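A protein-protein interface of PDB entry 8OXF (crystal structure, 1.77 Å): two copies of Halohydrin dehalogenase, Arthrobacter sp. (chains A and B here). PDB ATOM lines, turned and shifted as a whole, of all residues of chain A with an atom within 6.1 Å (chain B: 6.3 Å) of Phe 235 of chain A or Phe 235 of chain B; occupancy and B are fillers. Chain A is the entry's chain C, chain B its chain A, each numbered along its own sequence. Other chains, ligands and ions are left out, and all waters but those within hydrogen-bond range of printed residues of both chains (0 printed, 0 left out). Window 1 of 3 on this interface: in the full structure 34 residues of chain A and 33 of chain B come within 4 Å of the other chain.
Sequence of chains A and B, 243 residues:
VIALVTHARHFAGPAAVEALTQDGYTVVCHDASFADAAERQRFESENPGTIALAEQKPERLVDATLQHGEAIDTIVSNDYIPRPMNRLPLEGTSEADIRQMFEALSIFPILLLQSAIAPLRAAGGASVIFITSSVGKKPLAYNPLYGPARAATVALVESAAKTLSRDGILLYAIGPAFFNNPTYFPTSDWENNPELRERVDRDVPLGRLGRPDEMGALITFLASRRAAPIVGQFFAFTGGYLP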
ATOM      1  N   TYR A 172     -31.470  10.634  29.169  1.00  0.00           N
ATOM      2  CA  TYR A 172     -30.418  10.319  28.207  1.00  0.00           C
ATOM      3  C   TYR A 172     -29.739  11.597  27.756  1.00  0.00           C
ATOM      4  O   TYR A 172     -30.349  12.668  27.753  1.00  0.00           O
ATOM      5  CB  TYR A 172     -30.942   9.582  26.955  1.00  0.00           C
ATOM      6  CG  TYR A 172     -31.922   8.457  27.230  1.00  0.00           C
ATOM      7  CD1 TYR A 172     -33.273   8.717  27.425  1.00  0.00           C
ATOM      8  CD2 TYR A 172     -31.491   7.136  27.293  1.00  0.00           C
ATOM      9  CE1 TYR A 172     -34.168   7.687  27.679  1.00  0.00           C
ATOM     10  CE2 TYR A 172     -32.367   6.116  27.533  1.00  0.00           C
ATOM     11  CZ  TYR A 172     -33.713   6.396  27.722  1.00  0.00           C
ATOM     12  OH  TYR A 172     -34.605   5.371  27.978  1.00  0.00           O
ATOM     13  N   ALA A 173     -28.480  11.474  27.330  1.00  0.00           N
ATOM     14  CA  ALA A 173     -27.784  12.580  26.683  1.00  0.00           C
ATOM     15  C   ALA A 173     -27.353  12.142  25.295  1.00  0.00           C
ATOM     16  O   ALA A 173     -26.775  11.062  25.134  1.00  0.00           O
ATOM     17  CB  ALA A 173     -26.563  13.041  27.468  1.00  0.00           C
ATOM     18  N   ILE A 174     -27.663  12.960  24.306  1.00  0.00           N
ATOM     19  CA  ILE A 174     -27.157  12.798  22.944  1.00  0.00           C
ATOM     20  C   ILE A 174     -26.093  13.858  22.701  1.00  0.00           C
ATOM     21  O   ILE A 174     -26.285  15.035  23.045  1.00  0.00           O
ATOM     22  CB  ILE A 174     -28.296  12.929  21.921  1.00  0.00           C
ATOM     23  CG1 ILE A 174     -29.395  11.923  22.226  1.00  0.00           C
ATOM     24  CG2 ILE A 174     -27.770  12.762  20.510  1.00  0.00           C
ATOM     25  CD1 ILE A 174     -30.628  12.106  21.355  1.00  0.00           C
ATOM     26  N   GLY A 175     -24.989  13.453  22.078  1.00  0.00           N
ATOM     27  CA  GLY A 175     -23.880  14.350  21.831  1.00  0.00           C
ATOM     28  C   GLY A 175     -23.500  14.406  20.363  1.00  0.00           C
ATOM     29  O   GLY A 175     -22.668  13.633  19.878  1.00  0.00           O
ATOM     30  N   PRO A 176     -24.103  15.336  19.625  1.00  0.00           N
ATOM     31  CA  PRO A 176     -23.877  15.390  18.181  1.00  0.00           C
ATOM     32  C   PRO A 176     -22.572  16.079  17.845  1.00  0.00           C
ATOM     33  O   PRO A 176     -22.046  16.889  18.606  1.00  0.00           O
ATOM     34  CB  PRO A 176     -25.074  16.206  17.676  1.00  0.00           C
ATOM     35  CG  PRO A 176     -25.363  17.104  18.829  1.00  0.00           C
ATOM     36  CD  PRO A 176     -25.179  16.251  20.035  1.00  0.00           C
ATOM     37  N   LEU A 218     -33.402   8.540  16.345  1.00  0.00           N
ATOM     38  CA  LEU A 218     -32.862   8.245  17.666  1.00  0.00           C
ATOM     39  C   LEU A 218     -33.782   8.793  18.756  1.00  0.00           C
ATOM     40  O   LEU A 218     -34.108   8.085  19.717  1.00  0.00           O
ATOM     41  CB  LEU A 218     -31.440   8.800  17.796  1.00  0.00           C
ATOM     42  CG  LEU A 218     -30.836   8.726  19.194  1.00  0.00           C
ATOM     43  CD1 LEU A 218     -30.811   7.261  19.637  1.00  0.00           C
ATOM     44  CD2 LEU A 218     -29.430   9.299  19.180  1.00  0.00           C
ATOM     45  N   LEU A 222     -35.826   6.511  21.510  1.00  0.00           N
ATOM     46  CA  LEU A 222     -35.720   6.723  22.950  1.00  0.00           C
ATOM     47  C   LEU A 222     -37.075   7.062  23.558  1.00  0.00           C
ATOM     48  O   LEU A 222     -37.392   6.625  24.667  1.00  0.00           O
ATOM     49  CB  LEU A 222     -34.698   7.829  23.263  1.00  0.00           C
ATOM     50  CG  LEU A 222     -33.241   7.552  22.848  1.00  0.00           C
ATOM     51  CD1 LEU A 222     -32.307   8.726  23.169  1.00  0.00           C
ATOM     52  CD2 LEU A 222     -32.720   6.278  23.488  1.00  0.00           C
ATOM     53  N   ILE A 230     -31.132   1.001  28.489  1.00  0.00           N
ATOM     54  CA  ILE A 230     -30.002   1.835  28.066  1.00  0.00           C
ATOM     55  C   ILE A 230     -30.106   3.216  28.711  1.00  0.00           C
ATOM     56  O   ILE A 230     -29.416   4.152  28.294  1.00  0.00           O
ATOM     57  CB  ILE A 230     -29.882   1.943  26.523  1.00  0.00           C
ATOM     58  CG1 ILE A 230     -30.990   2.789  25.900  1.00  0.00           C
ATOM     59  CG2 ILE A 230     -29.804   0.540  25.875  1.00  0.00           C
ATOM     60  CD1 ILE A 230     -30.897   2.848  24.362  1.00  0.00           C
ATOM     61  N   VAL A 231     -30.950   3.351  29.746  1.00  0.00           N
ATOM     62  CA  VAL A 231     -31.162   4.645  30.389  1.00  0.00           C
ATOM     63  C   VAL A 231     -29.862   5.159  31.011  1.00  0.00           C
ATOM     64  O   VAL A 231     -29.002   4.385  31.441  1.00  0.00           O
ATOM     65  CB  VAL A 231     -32.270   4.532  31.454  1.00  0.00           C
ATOM     66  CG1 VAL A 231     -31.923   3.428  32.446  1.00  0.00           C
ATOM     67  CG2 VAL A 231     -32.474   5.849  32.198  1.00  0.00           C
ATOM     68  N   GLN A 233     -27.230   7.136  29.913  1.00  0.00           N
ATOM     69  CA  GLN A 233     -25.933   7.253  29.248  1.00  0.00           C
ATOM     70  C   GLN A 233     -25.955   8.329  28.172  1.00  0.00           C
ATOM     71  O   GLN A 233     -27.004   8.823  27.743  1.00  0.00           O
ATOM     72  CB  GLN A 233     -25.470   5.987  28.508  1.00  0.00           C
ATOM     73  CG  GLN A 233     -26.557   5.139  27.974  1.00  0.00           C
ATOM     74  CD  GLN A 233     -26.063   3.784  27.504  1.00  0.00           C
ATOM     75  OE1 GLN A 233     -24.865   3.586  27.235  1.00  0.00           O
ATOM     76  NE2 GLN A 233     -26.963   2.818  27.493  1.00  0.00           N
ATOM     77  N   PHE A 234     -24.751   8.560  27.675  1.00  0.00           N
ATOM     78  CA  PHE A 234     -24.446   9.471  26.583  1.00  0.00           C
ATOM     79  C   PHE A 234     -24.373   8.681  25.282  1.00  0.00           C
ATOM     80  O   PHE A 234     -23.692   7.651  25.223  1.00  0.00           O
ATOM     81  CB  PHE A 234     -23.115  10.153  26.898  1.00  0.00           C
ATOM     82  CG  PHE A 234     -22.547  10.990  25.781  1.00  0.00           C
ATOM     83  CD1 PHE A 234     -21.760  10.414  24.794  1.00  0.00           C
ATOM     84  CD2 PHE A 234     -22.749  12.363  25.762  1.00  0.00           C
ATOM     85  CE1 PHE A 234     -21.213  11.187  23.798  1.00  0.00           C
ATOM     86  CE2 PHE A 234     -22.201  13.143  24.779  1.00  0.00           C
ATOM     87  CZ  PHE A 234     -21.426  12.561  23.794  1.00  0.00           C
ATOM     88  N   PHE A 235     -25.064   9.158  24.240  1.00  0.00           N
ATOM     89  CA  PHE A 235     -24.970   8.573  22.900  1.00  0.00           C
ATOM     90  C   PHE A 235     -24.229   9.529  21.979  1.00  0.00           C
ATOM     91  O   PHE A 235     -24.697  10.647  21.735  1.00  0.00           O
ATOM     92  CB  PHE A 235     -26.346   8.253  22.314  1.00  0.00           C
ATOM     93  CG  PHE A 235     -27.162   7.375  23.197  1.00  0.00           C
ATOM     94  CD1 PHE A 235     -26.775   6.069  23.419  1.00  0.00           C
ATOM     95  CD2 PHE A 235     -28.273   7.874  23.859  1.00  0.00           C
ATOM     96  CE1 PHE A 235     -27.513   5.242  24.277  1.00  0.00           C
ATOM     97  CE2 PHE A 235     -29.019   7.055  24.722  1.00  0.00           C
ATOM     98  CZ  PHE A 235     -28.635   5.739  24.919  1.00  0.00           C
ATOM     99  N   ALA A 236     -23.088   9.084  21.458  1.00  0.00           N
ATOM    100  CA  ALA A 236     -22.443   9.838  20.390  1.00  0.00           C
ATOM    101  C   ALA A 236     -23.343   9.853  19.160  1.00  0.00           C
ATOM    102  O   ALA A 236     -23.842   8.811  18.731  1.00  0.00           O
ATOM    103  CB  ALA A 236     -21.091   9.219  20.039  1.00  0.00           C
ATOM    104  N   PHE A 237     -23.567  11.034  18.600  1.00  0.00           N
ATOM    105  CA  PHE A 237     -24.234  11.169  17.298  1.00  0.00           C
ATOM    106  C   PHE A 237     -23.250  11.888  16.383  1.00  0.00           C
ATOM    107  O   PHE A 237     -23.421  13.068  16.056  1.00  0.00           O
ATOM    108  CB  PHE A 237     -25.564  11.922  17.421  1.00  0.00           C
ATOM    109  CG  PHE A 237     -26.449  11.832  16.189  1.00  0.00           C
ATOM    110  CD1 PHE A 237     -27.346  10.806  16.030  1.00  0.00           C
ATOM    111  CD2 PHE A 237     -26.381  12.799  15.199  1.00  0.00           C
ATOM    112  CE1 PHE A 237     -28.166  10.730  14.918  1.00  0.00           C
ATOM    113  CE2 PHE A 237     -27.184  12.731  14.083  1.00  0.00           C
ATOM    114  CZ  PHE A 237     -28.084  11.693  13.941  1.00  0.00           C
ATOM    115  N   LEU B 171     -20.696  -0.823  12.765  1.00  0.00           N
ATOM    116  CA  LEU B 171     -20.329  -1.619  13.931  1.00  0.00           C
ATOM    117  C   LEU B 171     -20.848  -0.996  15.227  1.00  0.00           C
ATOM    118  O   LEU B 171     -20.799   0.222  15.405  1.00  0.00           O
ATOM    119  CB  LEU B 171     -18.807  -1.761  14.021  1.00  0.00           C
ATOM    120  CG  LEU B 171     -18.271  -3.021  13.336  1.00  0.00           C
ATOM    121  CD1 LEU B 171     -18.762  -3.132  11.885  1.00  0.00           C
ATOM    122  CD2 LEU B 171     -16.766  -3.143  13.460  1.00  0.00           C
ATOM    123  N   TYR B 172     -21.299  -1.848  16.152  1.00  0.00           N
ATOM    124  CA  TYR B 172     -21.800  -1.428  17.461  1.00  0.00           C
ATOM    125  C   TYR B 172     -21.421  -2.478  18.488  1.00  0.00           C
ATOM    126  O   TYR B 172     -21.325  -3.668  18.168  1.00  0.00           O
ATOM    127  CB  TYR B 172     -23.330  -1.274  17.501  1.00  0.00           C
ATOM    128  CG  TYR B 172     -23.921  -0.491  16.367  1.00  0.00           C
ATOM    129  CD1 TYR B 172     -24.080   0.892  16.471  1.00  0.00           C
ATOM    130  CD2 TYR B 172     -24.325  -1.122  15.184  1.00  0.00           C
ATOM    131  CE1 TYR B 172     -24.631   1.623  15.452  1.00  0.00           C
ATOM    132  CE2 TYR B 172     -24.882  -0.382  14.136  1.00  0.00           C
ATOM    133  CZ  TYR B 172     -25.028   0.998  14.283  1.00  0.00           C
ATOM    134  OH  TYR B 172     -25.553   1.779  13.254  1.00  0.00           O
ATOM    135  N   ALA B 173     -21.230  -2.034  19.731  1.00  0.00           N
ATOM    136  CA  ALA B 173     -21.041  -2.939  20.859  1.00  0.00           C
ATOM    137  C   ALA B 173     -22.143  -2.674  21.870  1.00  0.00           C
ATOM    138  O   ALA B 173     -22.444  -1.515  22.174  1.00  0.00           O
ATOM    139  CB  ALA B 173     -19.681  -2.753  21.535  1.00  0.00           C
ATOM    140  N   ILE B 174     -22.750  -3.742  22.365  1.00  0.00           N
ATOM    141  CA  ILE B 174     -23.721  -3.668  23.453  1.00  0.00           C
ATOM    142  C   ILE B 174     -23.113  -4.357  24.663  1.00  0.00           C
ATOM    143  O   ILE B 174     -22.571  -5.465  24.541  1.00  0.00           O
ATOM    144  CB  ILE B 174     -25.053  -4.325  23.063  1.00  0.00           C
ATOM    145  CG1 ILE B 174     -25.663  -3.651  21.837  1.00  0.00           C
ATOM    146  CG2 ILE B 174     -26.044  -4.271  24.209  1.00  0.00           C
ATOM    147  CD1 ILE B 174     -26.897  -4.371  21.401  1.00  0.00           C
ATOM    148  N   GLY B 175     -23.191  -3.708  25.824  1.00  0.00           N
ATOM    149  CA  GLY B 175     -22.569  -4.242  27.009  1.00  0.00           C
ATOM    150  C   GLY B 175     -23.560  -4.481  28.131  1.00  0.00           C
ATOM    151  O   GLY B 175     -23.778  -3.616  28.986  1.00  0.00           O
ATOM    152  N   PRO B 176     -24.160  -5.668  28.162  1.00  0.00           N
ATOM    153  CA  PRO B 176     -25.229  -5.942  29.135  1.00  0.00           C
ATOM    154  C   PRO B 176     -24.751  -6.223  30.554  1.00  0.00           C
ATOM    155  O   PRO B 176     -23.675  -6.780  30.794  1.00  0.00           O
ATOM    156  CB  PRO B 176     -25.909  -7.183  28.547  1.00  0.00           C
ATOM    157  CG  PRO B 176     -24.763  -7.901  27.895  1.00  0.00           C
ATOM    158  CD  PRO B 176     -23.979  -6.798  27.231  1.00  0.00           C
ATOM    159  N   LEU B 218     -33.462  -2.935  21.152  1.00  0.00           N
ATOM    160  CA  LEU B 218     -32.170  -2.326  20.819  1.00  0.00           C
ATOM    161  C   LEU B 218     -31.596  -2.920  19.527  1.00  0.00           C
ATOM    162  O   LEU B 218     -31.207  -2.185  18.610  1.00  0.00           O
ATOM    163  CB  LEU B 218     -31.187  -2.498  21.992  1.00  0.00           C
ATOM    164  CG  LEU B 218     -29.765  -1.960  21.753  1.00  0.00           C
ATOM    165  CD1 LEU B 218     -29.858  -0.520  21.301  1.00  0.00           C
ATOM    166  CD2 LEU B 218     -28.944  -2.030  23.042  1.00  0.00           C
ATOM    167  N   LEU B 222     -30.884  -1.003  15.897  1.00  0.00           N
ATOM    168  CA  LEU B 222     -29.572  -0.894  15.267  1.00  0.00           C
ATOM    169  C   LEU B 222     -29.599  -1.480  13.859  1.00  0.00           C
ATOM    170  O   LEU B 222     -29.087  -0.868  12.910  1.00  0.00           O
ATOM    171  CB  LEU B 222     -28.517  -1.570  16.145  1.00  0.00           C
ATOM    172  CG  LEU B 222     -28.344  -0.884  17.503  1.00  0.00           C
ATOM    173  CD1 LEU B 222     -27.339  -1.629  18.373  1.00  0.00           C
ATOM    174  CD2 LEU B 222     -27.925   0.580  17.316  1.00  0.00           C
ATOM    175  N   ILE B 230     -24.853   6.972  15.009  1.00  0.00           N
ATOM    176  CA  ILE B 230     -24.379   6.533  16.320  1.00  0.00           C
ATOM    177  C   ILE B 230     -23.441   5.338  16.137  1.00  0.00           C
ATOM    178  O   ILE B 230     -23.090   4.657  17.110  1.00  0.00           O
ATOM    179  CB  ILE B 230     -25.537   6.220  17.301  1.00  0.00           C
ATOM    180  CG1 ILE B 230     -26.325   4.959  16.897  1.00  0.00           C
ATOM    181  CG2 ILE B 230     -26.477   7.420  17.443  1.00  0.00           C
ATOM    182  CD1 ILE B 230     -27.528   4.646  17.833  1.00  0.00           C
ATOM    183  N   VAL B 231     -22.971   5.119  14.902  1.00  0.00           N
ATOM    184  CA  VAL B 231     -22.085   3.993  14.626  1.00  0.00           C
ATOM    185  C   VAL B 231     -20.796   4.072  15.445  1.00  0.00           C
ATOM    186  O   VAL B 231     -20.275   5.157  15.736  1.00  0.00           O
ATOM    187  CB  VAL B 231     -21.760   3.934  13.122  1.00  0.00           C
ATOM    188  CG1 VAL B 231     -21.080   5.220  12.682  1.00  0.00           C
ATOM    189  CG2 VAL B 231     -20.867   2.738  12.805  1.00  0.00           C
ATOM    190  N   GLY B 232     -20.295   2.898  15.831  1.00  0.00           N
ATOM    191  CA  GLY B 232     -18.937   2.753  16.313  1.00  0.00           C
ATOM    192  C   GLY B 232     -18.761   2.996  17.788  1.00  0.00           C
ATOM    193  O   GLY B 232     -17.685   3.453  18.211  1.00  0.00           O
ATOM    194  N   GLN B 233     -19.781   2.716  18.591  1.00  0.00           N
ATOM    195  CA  GLN B 233     -19.716   3.022  20.008  1.00  0.00           C
ATOM    196  C   GLN B 233     -20.346   1.903  20.812  1.00  0.00           C
ATOM    197  O   GLN B 233     -21.002   0.992  20.281  1.00  0.00           O
ATOM    198  CB  GLN B 233     -20.392   4.357  20.351  1.00  0.00           C
ATOM    199  CG  GLN B 233     -21.910   4.311  20.459  1.00  0.00           C
ATOM    200  CD  GLN B 233     -22.501   5.711  20.710  1.00  0.00           C
ATOM    201  OE1 GLN B 233     -22.366   6.283  21.803  1.00  0.00           O
ATOM    202  NE2 GLN B 233     -23.125   6.274  19.689  1.00  0.00           N
ATOM    203  N   PHE B 234     -20.144   2.034  22.119  1.00  0.00           N
ATOM    204  CA  PHE B 234     -20.542   1.070  23.128  1.00  0.00           C
ATOM    205  C   PHE B 234     -21.824   1.550  23.790  1.00  0.00           C
ATOM    206  O   PHE B 234     -21.897   2.697  24.236  1.00  0.00           O
ATOM    207  CB  PHE B 234     -19.404   0.947  24.142  1.00  0.00           C
ATOM    208  CG  PHE B 234     -19.737   0.144  25.376  1.00  0.00           C
ATOM    209  CD1 PHE B 234     -20.312   0.739  26.487  1.00  0.00           C
ATOM    210  CD2 PHE B 234     -19.420  -1.199  25.424  1.00  0.00           C
ATOM    211  CE1 PHE B 234     -20.577  -0.007  27.613  1.00  0.00           C
ATOM    212  CE2 PHE B 234     -19.676  -1.945  26.553  1.00  0.00           C
ATOM    213  CZ  PHE B 234     -20.245  -1.354  27.642  1.00  0.00           C
ATOM    214  N   PHE B 235     -22.836   0.687  23.835  1.00  0.00           N
ATOM    215  CA  PHE B 235     -24.106   1.000  24.480  1.00  0.00           C
ATOM    216  C   PHE B 235     -24.226   0.175  25.758  1.00  0.00           C
ATOM    217  O   PHE B 235     -24.320  -1.061  25.709  1.00  0.00           O
ATOM    218  CB  PHE B 235     -25.291   0.739  23.553  1.00  0.00           C
ATOM    219  CG  PHE B 235     -25.214   1.468  22.238  1.00  0.00           C
ATOM    220  CD1 PHE B 235     -25.438   2.841  22.172  1.00  0.00           C
ATOM    221  CD2 PHE B 235     -24.938   0.781  21.064  1.00  0.00           C
ATOM    222  CE1 PHE B 235     -25.371   3.529  20.958  1.00  0.00           C
ATOM    223  CE2 PHE B 235     -24.884   1.457  19.847  1.00  0.00           C
ATOM    224  CZ  PHE B 235     -25.097   2.841  19.799  1.00  0.00           C
ATOM    225  N   ALA B 236     -24.231   0.850  26.900  1.00  0.00           N
ATOM    226  CA  ALA B 236     -24.526   0.151  28.143  1.00  0.00           C
ATOM    227  C   ALA B 236     -25.972  -0.344  28.106  1.00  0.00           C
ATOM    228  O   ALA B 236     -26.874   0.384  27.679  1.00  0.00           O
ATOM    229  CB  ALA B 236     -24.276   1.064  29.346  1.00  0.00           C
ATOM    230  N   PHE B 237     -26.184  -1.620  28.491  1.00  0.00           N
ATOM    231  CA  PHE B 237     -27.528  -2.202  28.620  1.00  0.00           C
ATOM    232  C   PHE B 237     -27.611  -2.747  30.043  1.00  0.00           C
ATOM    233  O   PHE B 237     -27.494  -3.958  30.264  1.00  0.00           O
ATOM    234  CB  PHE B 237     -27.802  -3.298  27.558  1.00  0.00           C
ATOM    235  CG  PHE B 237     -29.234  -3.782  27.545  1.00  0.00           C
ATOM    236  CD1 PHE B 237     -29.647  -4.827  28.370  1.00  0.00           C
ATOM    237  CD2 PHE B 237     -30.167  -3.195  26.715  1.00  0.00           C
ATOM    238  CE1 PHE B 237     -30.966  -5.262  28.367  1.00  0.00           C
ATOM    239  CE2 PHE B 237     -31.479  -3.634  26.697  1.00  0.00           C
ATOM    240  CZ  PHE B 237     -31.878  -4.665  27.522  1.00  0.00           C
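The backbone carbonyl oxygen of Gln 233 of chain B is in hydrogen-bond range of the backbone NH of Ala 173 of chain B (3.1 Å).
The backbone carbonyl oxygen of Phe 235 of chain B sits at hydrogen-bond distance from the backbone NH of Gly 175 of chain B, at 2.9 Å.
O of Ile 230 of chain B lies within hydrogen-bond range of NE2 of Gln 233 of chain B, 3.0 Å away.
The backbone carbonyl oxygen of Gln 233 of chain A is in hydrogen-bond range of the backbone NH of Ala 173 of chain A, at 3.1 Å.
O of Phe 235 of chain A lies within hydrogen-bond range of N of Gly 175 of chain A (2.8 Å).
O of Gly 175 of chain A sits at hydrogen-bond distance from N of Phe 237 of chain A (3.0 Å).
NE2 of Gln 233 of chain B is in hydrogen-bond range of O of Ala 236 of chain A, at 2.8 Å.
The backbone carbonyl oxygen (O) of Ala 236 of chain B sits at hydrogen-bond distance from the side-chain amide nitrogen (NE2) of Gln 233 of chain A.
Leu 218 of chain A touches Ile 230 of chain B, and with the chains exchanged Ile 230 of chain A touches Leu 218 of chain B.
Gln 233 of chain A touches Phe 235 of chain B, and with the chains exchanged Phe 235 of chain A touches Gln 233 of chain B.
Phe 234 of chain A touches Gln 233 of chain B, but with the chains exchanged Gln 233 of chain A does not touch Phe 234 of chain B (4.3 Å).
Phe 235 of chain B touches its own counterpart, Phe 235 of chain A.
Among the printed residues, pairs that only touch across the chains: Ala 236 of chain A with Ile 230 of chain B, Ile 230 of chain A with Ala 236 of chain B, Phe 235 of chain A with Gln 233 of chain B, Phe 235 of chain A with Phe 235 of chain B, Phe 237 of chain A with Ile 230 of chain B, Gln 233 of chain A with Phe 235 of chain B, Ile 230 of chain A with Phe 237 of chain B, Leu 218 of chain A with Ile 230 of chain B, Phe 234 of chain A with Gln 233 of chain B and Ile 230 of chain A with Leu 218 of chain B.
Of the 14 printed residues of chain A, 7 touch a printed residue of chain B.
Along chain A the printed residues that touch a printed residue of chain B span positions 218 to 237.
Hydrophobic or aromatic side chains of chain B that line the printed part of chain A: Leu 218, Ile 230, Phe 235, Ala 236 and Phe 237.
Of chain B, only Gln 233 and Phe 235 come within 4 Å of Phe 235 of chain A.
Of chain A, only Gln 233 and Phe 235 come within 4 Å of Phe 235 of chain B.
Printed residues of chain A within 4 Å of Ile 230 of chain B: Leu 218 (3.9 Å), Ala 236 (3.2 Å) and Phe 237 (3.8 Å).
Printed residues of chain A within 4 Å of Leu 218 of chain B: Ile 230.
The nearest residue of chain B that does not touch Phe 235 of chain A is Ile 230 of chain B (4.9 Å).
The nearest residue of chain A that does not touch Phe 235 of chain B is Ile 230 of chain A (5.1 Å).
The nearest printed residue of chain B that does not touch Gln 233 of chain A is Phe 234 of chain B (4.3 Å).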
